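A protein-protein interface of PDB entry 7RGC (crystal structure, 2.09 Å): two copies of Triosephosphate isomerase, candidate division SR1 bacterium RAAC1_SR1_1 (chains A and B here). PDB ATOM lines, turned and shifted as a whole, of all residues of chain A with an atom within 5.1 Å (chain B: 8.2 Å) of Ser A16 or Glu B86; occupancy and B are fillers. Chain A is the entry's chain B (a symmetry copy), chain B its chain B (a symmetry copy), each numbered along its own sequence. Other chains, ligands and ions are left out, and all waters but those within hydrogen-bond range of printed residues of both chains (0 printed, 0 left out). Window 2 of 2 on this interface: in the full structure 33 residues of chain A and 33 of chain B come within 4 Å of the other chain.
OG of Ser A16 lies close to N of Lys A18 (3.3 Å). The backbone NH (N) of Asp A19 sits at hydrogen-bond distance from the side-chain hydroxyl (OG) of Ser A16 (3.1 Å). The side-chain hydroxyl of Ser B52 is in hydrogen-bond range of the backbone carbonyl oxygen of Leu B87, at 2.6 Å.
Of the 15 printed residues of chain B, 3 touch a printed residue of chain A. Printed residues of chain B that touch a printed residue of chain A: Ile B83, Glu B86 and Leu B87. Of the 8 printed residues of chain A, 3 touch a printed residue of chain B. Printed residues of chain A that touch a printed residue of chain B: Lys A15, Ser A16 and His A17. Hydrophobic or aromatic side chains of chain A that line the printed part of chain B: His A17. Along chain A the printed residues that touch a printed residue of chain B span positions 15 to 17. Among the printed residues, 6 pairs touch across the chains. Among the printed residues, no Asp or Glu carboxylate lies within 4 Å of a Lys or Arg side-chain nitrogen of the other chain.
The backbone NH of His A17 is in hydrogen-bond range of the side-chain carboxylate of Glu B86, 2.9 Å away.
No position is printed for both chains. Of the 6 pairs that touch across the chains among the printed residues, none has its exchanged pair printed and touching as well.
Among the printed residues, pairs that only touch across the chains: Lys A15 with Ile B83, Ser A16 with Ile B83, Ser A16 with Glu B86, His A17 with Ile B83 and His A17 with Leu B87.
Ser A16 touches two residues of chain B. Of the printed residues of chain A, Glu B86 touches Ser A16 (3.5 Å) and His A17 (2.9 Å). Of the printed residues of chain B, His A17 touches Ile B83, Glu B86 and Leu B87. Of the printed residues of chain A, Leu B87 touches His A17 (3.5 Å). Of the printed residues of chain B, Lys A15 touches Ile B83. Of the printed residues of chain A, Ile B83 touches Lys A15 (3.6 Å), Ser A16 (3.5 Å) and His A17 (3.9 Å). Gln A21 touches none of the printed residues of chain B. The nearest residue of chain B that does not touch Ser A16 is Leu B82 (6.0 Å). The nearest printed residue of chain A that does not touch Glu B86 is Lys A18 (4.01 Å). The nearest printed residue of chain B that does not touch His A17 is Leu B82 (6.7 Å).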
ATOM      1  N   TYR A  14       9.085  11.282 -21.441  1.00  0.00           N
ATOM      2  CA  TYR A  14       9.773  10.680 -20.312  1.00  0.00           C
ATOM      3  C   TYR A  14      11.235  10.436 -20.656  1.00  0.00           C
ATOM      4  O   TYR A  14      11.574  10.156 -21.812  1.00  0.00           O
ATOM      5  CB  TYR A  14       9.129   9.355 -19.902  1.00  0.00           C
ATOM      6  CG  TYR A  14       7.902   9.482 -19.038  1.00  0.00           C
ATOM      7  CD1 TYR A  14       6.639   9.536 -19.607  1.00  0.00           C
ATOM      8  CD2 TYR A  14       8.004   9.526 -17.652  1.00  0.00           C
ATOM      9  CE1 TYR A  14       5.503   9.630 -18.822  1.00  0.00           C
ATOM     10  CE2 TYR A  14       6.876   9.635 -16.856  1.00  0.00           C
ATOM     11  CZ  TYR A  14       5.627   9.683 -17.448  1.00  0.00           C
ATOM     12  OH  TYR A  14       4.498   9.786 -16.666  1.00  0.00           O
ATOM     13  N   LYS A  15      12.086  10.560 -19.625  1.00  0.00           N
ATOM     14  CA  LYS A  15      13.481  10.116 -19.564  1.00  0.00           C
ATOM     15  C   LYS A  15      14.456  11.235 -19.914  1.00  0.00           C
ATOM     16  O   LYS A  15      14.484  11.715 -21.054  1.00  0.00           O
ATOM     17  CB  LYS A  15      13.743   8.897 -20.470  1.00  0.00           C
ATOM     18  CG  LYS A  15      12.894   7.666 -20.152  1.00  0.00           C
ATOM     19  CD  LYS A  15      13.462   6.384 -20.804  1.00  0.00           C
ATOM     20  CE  LYS A  15      12.590   5.170 -20.512  1.00  0.00           C
ATOM     21  NZ  LYS A  15      12.516   4.857 -19.061  1.00  0.00           N
ATOM     22  N   SER A  16      15.265  11.648 -18.934  1.00  0.00           N
ATOM     23  CA  SER A  16      16.463  12.436 -19.210  1.00  0.00           C
ATOM     24  C   SER A  16      17.390  11.683 -20.171  1.00  0.00           C
ATOM     25  O   SER A  16      17.147  10.533 -20.535  1.00  0.00           O
ATOM     26  CB  SER A  16      17.214  12.747 -17.915  1.00  0.00           C
ATOM     27  OG  SER A  16      17.828  11.580 -17.389  1.00  0.00           O
ATOM     28  N   HIS A  17      18.467  12.352 -20.596  1.00  0.00           N
ATOM     29  CA  HIS A  17      19.461  11.663 -21.421  1.00  0.00           C
ATOM     30  C   HIS A  17      20.105  10.507 -20.671  1.00  0.00           C
ATOM     31  O   HIS A  17      20.412   9.473 -21.280  1.00  0.00           O
ATOM     32  CB  HIS A  17      20.541  12.632 -21.913  1.00  0.00           C
ATOM     33  CG  HIS A  17      20.131  13.417 -23.120  1.00  0.00           C
ATOM     34  ND1 HIS A  17      20.186  12.901 -24.397  1.00  0.00           N
ATOM     35  CD2 HIS A  17      19.637  14.674 -23.245  1.00  0.00           C
ATOM     36  CE1 HIS A  17      19.746  13.804 -25.256  1.00  0.00           C
ATOM     37  NE2 HIS A  17      19.407  14.889 -24.583  1.00  0.00           N
ATOM     38  N   LYS A  18      20.311  10.656 -19.356  1.00  0.00           N
ATOM     39  CA  LYS A  18      20.892   9.561 -18.578  1.00  0.00           C
ATOM     40  C   LYS A  18      19.905   8.403 -18.439  1.00  0.00           C
ATOM     41  O   LYS A  18      20.295   7.234 -18.537  1.00  0.00           O
ATOM     42  CB  LYS A  18      21.345  10.058 -17.203  1.00  0.00           C
ATOM     43  N   ASP A  19      18.630   8.707 -18.205  1.00  0.00           N
ATOM     44  CA  ASP A  19      17.623   7.653 -18.178  1.00  0.00           C
ATOM     45  C   ASP A  19      17.591   6.890 -19.494  1.00  0.00           C
ATOM     46  O   ASP A  19      17.438   5.663 -19.500  1.00  0.00           O
ATOM     47  CB  ASP A  19      16.233   8.231 -17.894  1.00  0.00           C
ATOM     48  CG  ASP A  19      16.096   8.796 -16.494  1.00  0.00           C
ATOM     49  OD1 ASP A  19      16.833   8.352 -15.587  1.00  0.00           O
ATOM     50  OD2 ASP A  19      15.224   9.674 -16.309  1.00  0.00           O
ATOM     51  N   LEU A  20      17.708   7.602 -20.621  1.00  0.00           N
ATOM     52  CA  LEU A  20      17.645   6.944 -21.923  1.00  0.00           C
ATOM     53  C   LEU A  20      18.878   6.071 -22.153  1.00  0.00           C
ATOM     54  O   LEU A  20      18.769   4.939 -22.641  1.00  0.00           O
ATOM     55  CB  LEU A  20      17.497   7.992 -23.028  1.00  0.00           C
ATOM     56  CG  LEU A  20      17.152   7.520 -24.443  1.00  0.00           C
ATOM     57  CD1 LEU A  20      15.793   6.823 -24.480  1.00  0.00           C
ATOM     58  CD2 LEU A  20      17.195   8.655 -25.446  1.00  0.00           C
ATOM     59  N   GLN A  21      20.057   6.572 -21.783  1.00  0.00           N
ATOM     60  CA  GLN A  21      21.267   5.765 -21.892  1.00  0.00           C
ATOM     61  C   GLN A  21      21.170   4.513 -21.031  1.00  0.00           C
ATOM     62  O   GLN A  21      21.446   3.407 -21.502  1.00  0.00           O
ATOM     63  CB  GLN A  21      22.494   6.603 -21.518  1.00  0.00           C
ATOM     64  N   SER B  52      23.390  21.674 -29.614  1.00  0.00           N
ATOM     65  CA  SER B  52      23.971  21.704 -28.272  1.00  0.00           C
ATOM     66  C   SER B  52      25.488  21.488 -28.287  1.00  0.00           C
ATOM     67  O   SER B  52      26.233  22.164 -27.566  1.00  0.00           O
ATOM     68  CB  SER B  52      23.278  20.625 -27.428  1.00  0.00           C
ATOM     69  OG  SER B  52      23.615  20.691 -26.061  1.00  0.00           O
ATOM     70  N   LEU B  62      22.000  28.552 -26.911  1.00  0.00           N
ATOM     71  CA  LEU B  62      20.999  27.655 -27.470  1.00  0.00           C
ATOM     72  C   LEU B  62      19.594  28.078 -27.039  1.00  0.00           C
ATOM     73  O   LEU B  62      19.326  28.247 -25.844  1.00  0.00           O
ATOM     74  CB  LEU B  62      21.274  26.221 -27.022  1.00  0.00           C
ATOM     75  CG  LEU B  62      20.483  25.076 -27.687  1.00  0.00           C
ATOM     76  CD1 LEU B  62      20.735  25.041 -29.184  1.00  0.00           C
ATOM     77  CD2 LEU B  62      20.848  23.726 -27.068  1.00  0.00           C
ATOM     78  N   ASP B  71       7.356  18.624 -16.347  1.00  0.00           N
ATOM     79  CA  ASP B  71       8.698  18.051 -16.390  1.00  0.00           C
ATOM     80  C   ASP B  71       8.702  16.718 -17.134  1.00  0.00           C
ATOM     81  O   ASP B  71       9.611  16.442 -17.923  1.00  0.00           O
ATOM     82  CB  ASP B  71       9.237  17.877 -14.974  1.00  0.00           C
ATOM     83  CG  ASP B  71       9.814  19.165 -14.403  1.00  0.00           C
ATOM     84  OD1 ASP B  71       9.407  20.267 -14.844  1.00  0.00           O
ATOM     85  OD2 ASP B  71      10.699  19.064 -13.522  1.00  0.00           O
ATOM     86  N   GLN B  72       7.690  15.892 -16.901  1.00  0.00           N
ATOM     87  CA  GLN B  72       7.537  14.616 -17.586  1.00  0.00           C
ATOM     88  C   GLN B  72       6.076  14.219 -17.506  1.00  0.00           C
ATOM     89  O   GLN B  72       5.345  14.680 -16.631  1.00  0.00           O
ATOM     90  CB  GLN B  72       8.422  13.532 -16.961  1.00  0.00           C
ATOM     91  N   SER B  80      10.502  18.062 -22.991  1.00  0.00           N
ATOM     92  CA  SER B  80      10.469  18.409 -21.575  1.00  0.00           C
ATOM     93  C   SER B  80      11.510  19.480 -21.254  1.00  0.00           C
ATOM     94  O   SER B  80      12.627  19.441 -21.784  1.00  0.00           O
ATOM     95  CB  SER B  80      10.730  17.178 -20.716  1.00  0.00           C
ATOM     96  OG  SER B  80      11.122  17.541 -19.405  1.00  0.00           O
ATOM     97  N   PRO B  81      11.156  20.443 -20.391  1.00  0.00           N
ATOM     98  CA  PRO B  81      12.150  21.445 -19.970  1.00  0.00           C
ATOM     99  C   PRO B  81      13.383  20.820 -19.350  1.00  0.00           C
ATOM    100  O   PRO B  81      14.480  21.377 -19.486  1.00  0.00           O
ATOM    101  CB  PRO B  81      11.391  22.306 -18.947  1.00  0.00           C
ATOM    102  CG  PRO B  81       9.953  21.928 -19.071  1.00  0.00           C
ATOM    103  CD  PRO B  81       9.857  20.601 -19.711  1.00  0.00           C
ATOM    104  N   LEU B  82      13.234  19.673 -18.673  1.00  0.00           N
ATOM    105  CA  LEU B  82      14.391  19.006 -18.094  1.00  0.00           C
ATOM    106  C   LEU B  82      15.429  18.695 -19.159  1.00  0.00           C
ATOM    107  O   LEU B  82      16.629  18.762 -18.897  1.00  0.00           O
ATOM    108  CB  LEU B  82      13.966  17.724 -17.384  1.00  0.00           C
ATOM    109  CG  LEU B  82      13.222  17.914 -16.067  1.00  0.00           C
ATOM    110  CD1 LEU B  82      13.149  16.588 -15.346  1.00  0.00           C
ATOM    111  CD2 LEU B  82      13.941  18.928 -15.226  1.00  0.00           C
ATOM    112  N   ILE B  83      14.985  18.367 -20.372  1.00  0.00           N
ATOM    113  CA  ILE B  83      15.928  18.018 -21.431  1.00  0.00           C
ATOM    114  C   ILE B  83      16.569  19.273 -22.000  1.00  0.00           C
ATOM    115  O   ILE B  83      17.763  19.287 -22.319  1.00  0.00           O
ATOM    116  CB  ILE B  83      15.234  17.197 -22.536  1.00  0.00           C
ATOM    117  CG1 ILE B  83      14.700  15.882 -21.977  1.00  0.00           C
ATOM    118  CG2 ILE B  83      16.211  16.924 -23.665  1.00  0.00           C
ATOM    119  CD1 ILE B  83      15.781  14.997 -21.469  1.00  0.00           C
ATOM    120  N   LEU B  84      15.784  20.339 -22.167  1.00  0.00           N
ATOM    121  CA  LEU B  84      16.371  21.602 -22.596  1.00  0.00           C
ATOM    122  C   LEU B  84      17.421  22.082 -21.602  1.00  0.00           C
ATOM    123  O   LEU B  84      18.458  22.629 -21.997  1.00  0.00           O
ATOM    124  CB  LEU B  84      15.277  22.657 -22.776  1.00  0.00           C
ATOM    125  CG  LEU B  84      14.205  22.209 -23.773  1.00  0.00           C
ATOM    126  CD1 LEU B  84      13.243  23.356 -24.058  1.00  0.00           C
ATOM    127  CD2 LEU B  84      14.864  21.678 -25.053  1.00  0.00           C
ATOM    128  N   LYS B  85      17.167  21.895 -20.303  1.00  0.00           N
ATOM    129  CA  LYS B  85      18.174  22.261 -19.313  1.00  0.00           C
ATOM    130  C   LYS B  85      19.422  21.411 -19.492  1.00  0.00           C
ATOM    131  O   LYS B  85      20.543  21.930 -19.484  1.00  0.00           O
ATOM    132  CB  LYS B  85      17.607  22.117 -17.898  1.00  0.00           C
ATOM    133  N   GLU B  86      19.237  20.105 -19.710  1.00  0.00           N
ATOM    134  CA  GLU B  86      20.362  19.204 -19.929  1.00  0.00           C
ATOM    135  C   GLU B  86      21.216  19.648 -21.109  1.00  0.00           C
ATOM    136  O   GLU B  86      22.447  19.592 -21.045  1.00  0.00           O
ATOM    137  CB  GLU B  86      19.847  17.784 -20.166  1.00  0.00           C
ATOM    138  CG  GLU B  86      19.729  16.918 -18.924  1.00  0.00           C
ATOM    139  CD  GLU B  86      19.560  15.451 -19.277  1.00  0.00           C
ATOM    140  OE1 GLU B  86      18.861  15.161 -20.276  1.00  0.00           O
ATOM    141  OE2 GLU B  86      20.139  14.588 -18.577  1.00  0.00           O
ATOM    142  N   LEU B  87      20.588  20.086 -22.200  1.00  0.00           N
ATOM    143  CA  LEU B  87      21.360  20.460 -23.381  1.00  0.00           C
ATOM    144  C   LEU B  87      21.971  21.854 -23.296  1.00  0.00           C
ATOM    145  O   LEU B  87      22.656  22.263 -24.241  1.00  0.00           O
ATOM    146  CB  LEU B  87      20.492  20.381 -24.633  1.00  0.00           C
ATOM    147  CG  LEU B  87      19.849  19.051 -24.997  1.00  0.00           C
ATOM    148  CD1 LEU B  87      18.905  19.274 -26.166  1.00  0.00           C
ATOM    149  CD2 LEU B  87      20.911  18.004 -25.333  1.00  0.00           C
ATOM    150  N   GLY B  88      21.739  22.600 -22.216  1.00  0.00           N
ATOM    151  CA  GLY B  88      22.249  23.959 -22.143  1.00  0.00           C
ATOM    152  C   GLY B  88      21.386  24.998 -22.834  1.00  0.00           C
ATOM    153  O   GLY B  88      21.874  26.086 -23.147  1.00  0.00           O
ATOM    154  N   ALA B  89      20.123  24.691 -23.117  1.00  0.00           N
ATOM    155  CA  ALA B  89      19.233  25.702 -23.669  1.00  0.00           C
ATOM    156  C   ALA B  89      19.038  26.812 -22.643  1.00  0.00           C
ATOM    157  O   ALA B  89      18.703  26.552 -21.485  1.00  0.00           O
ATOM    158  CB  ALA B  89      17.892  25.073 -24.058  1.00  0.00           C
ATOM    159  N   ILE B 122      15.086  28.812 -17.384  1.00  0.00           N
ATOM    160  CA  ILE B 122      15.204  29.036 -18.817  1.00  0.00           C
ATOM    161  C   ILE B 122      14.579  30.383 -19.123  1.00  0.00           C
ATOM    162  O   ILE B 122      13.491  30.695 -18.625  1.00  0.00           O
ATOM    163  CB  ILE B 122      14.536  27.913 -19.621  1.00  0.00           C
ATOM    164  CG1 ILE B 122      15.114  26.566 -19.192  1.00  0.00           C
ATOM    165  CG2 ILE B 122      14.761  28.145 -21.105  1.00  0.00           C
ATOM    166  CD1 ILE B 122      14.315  25.386 -19.638  1.00  0.00           C
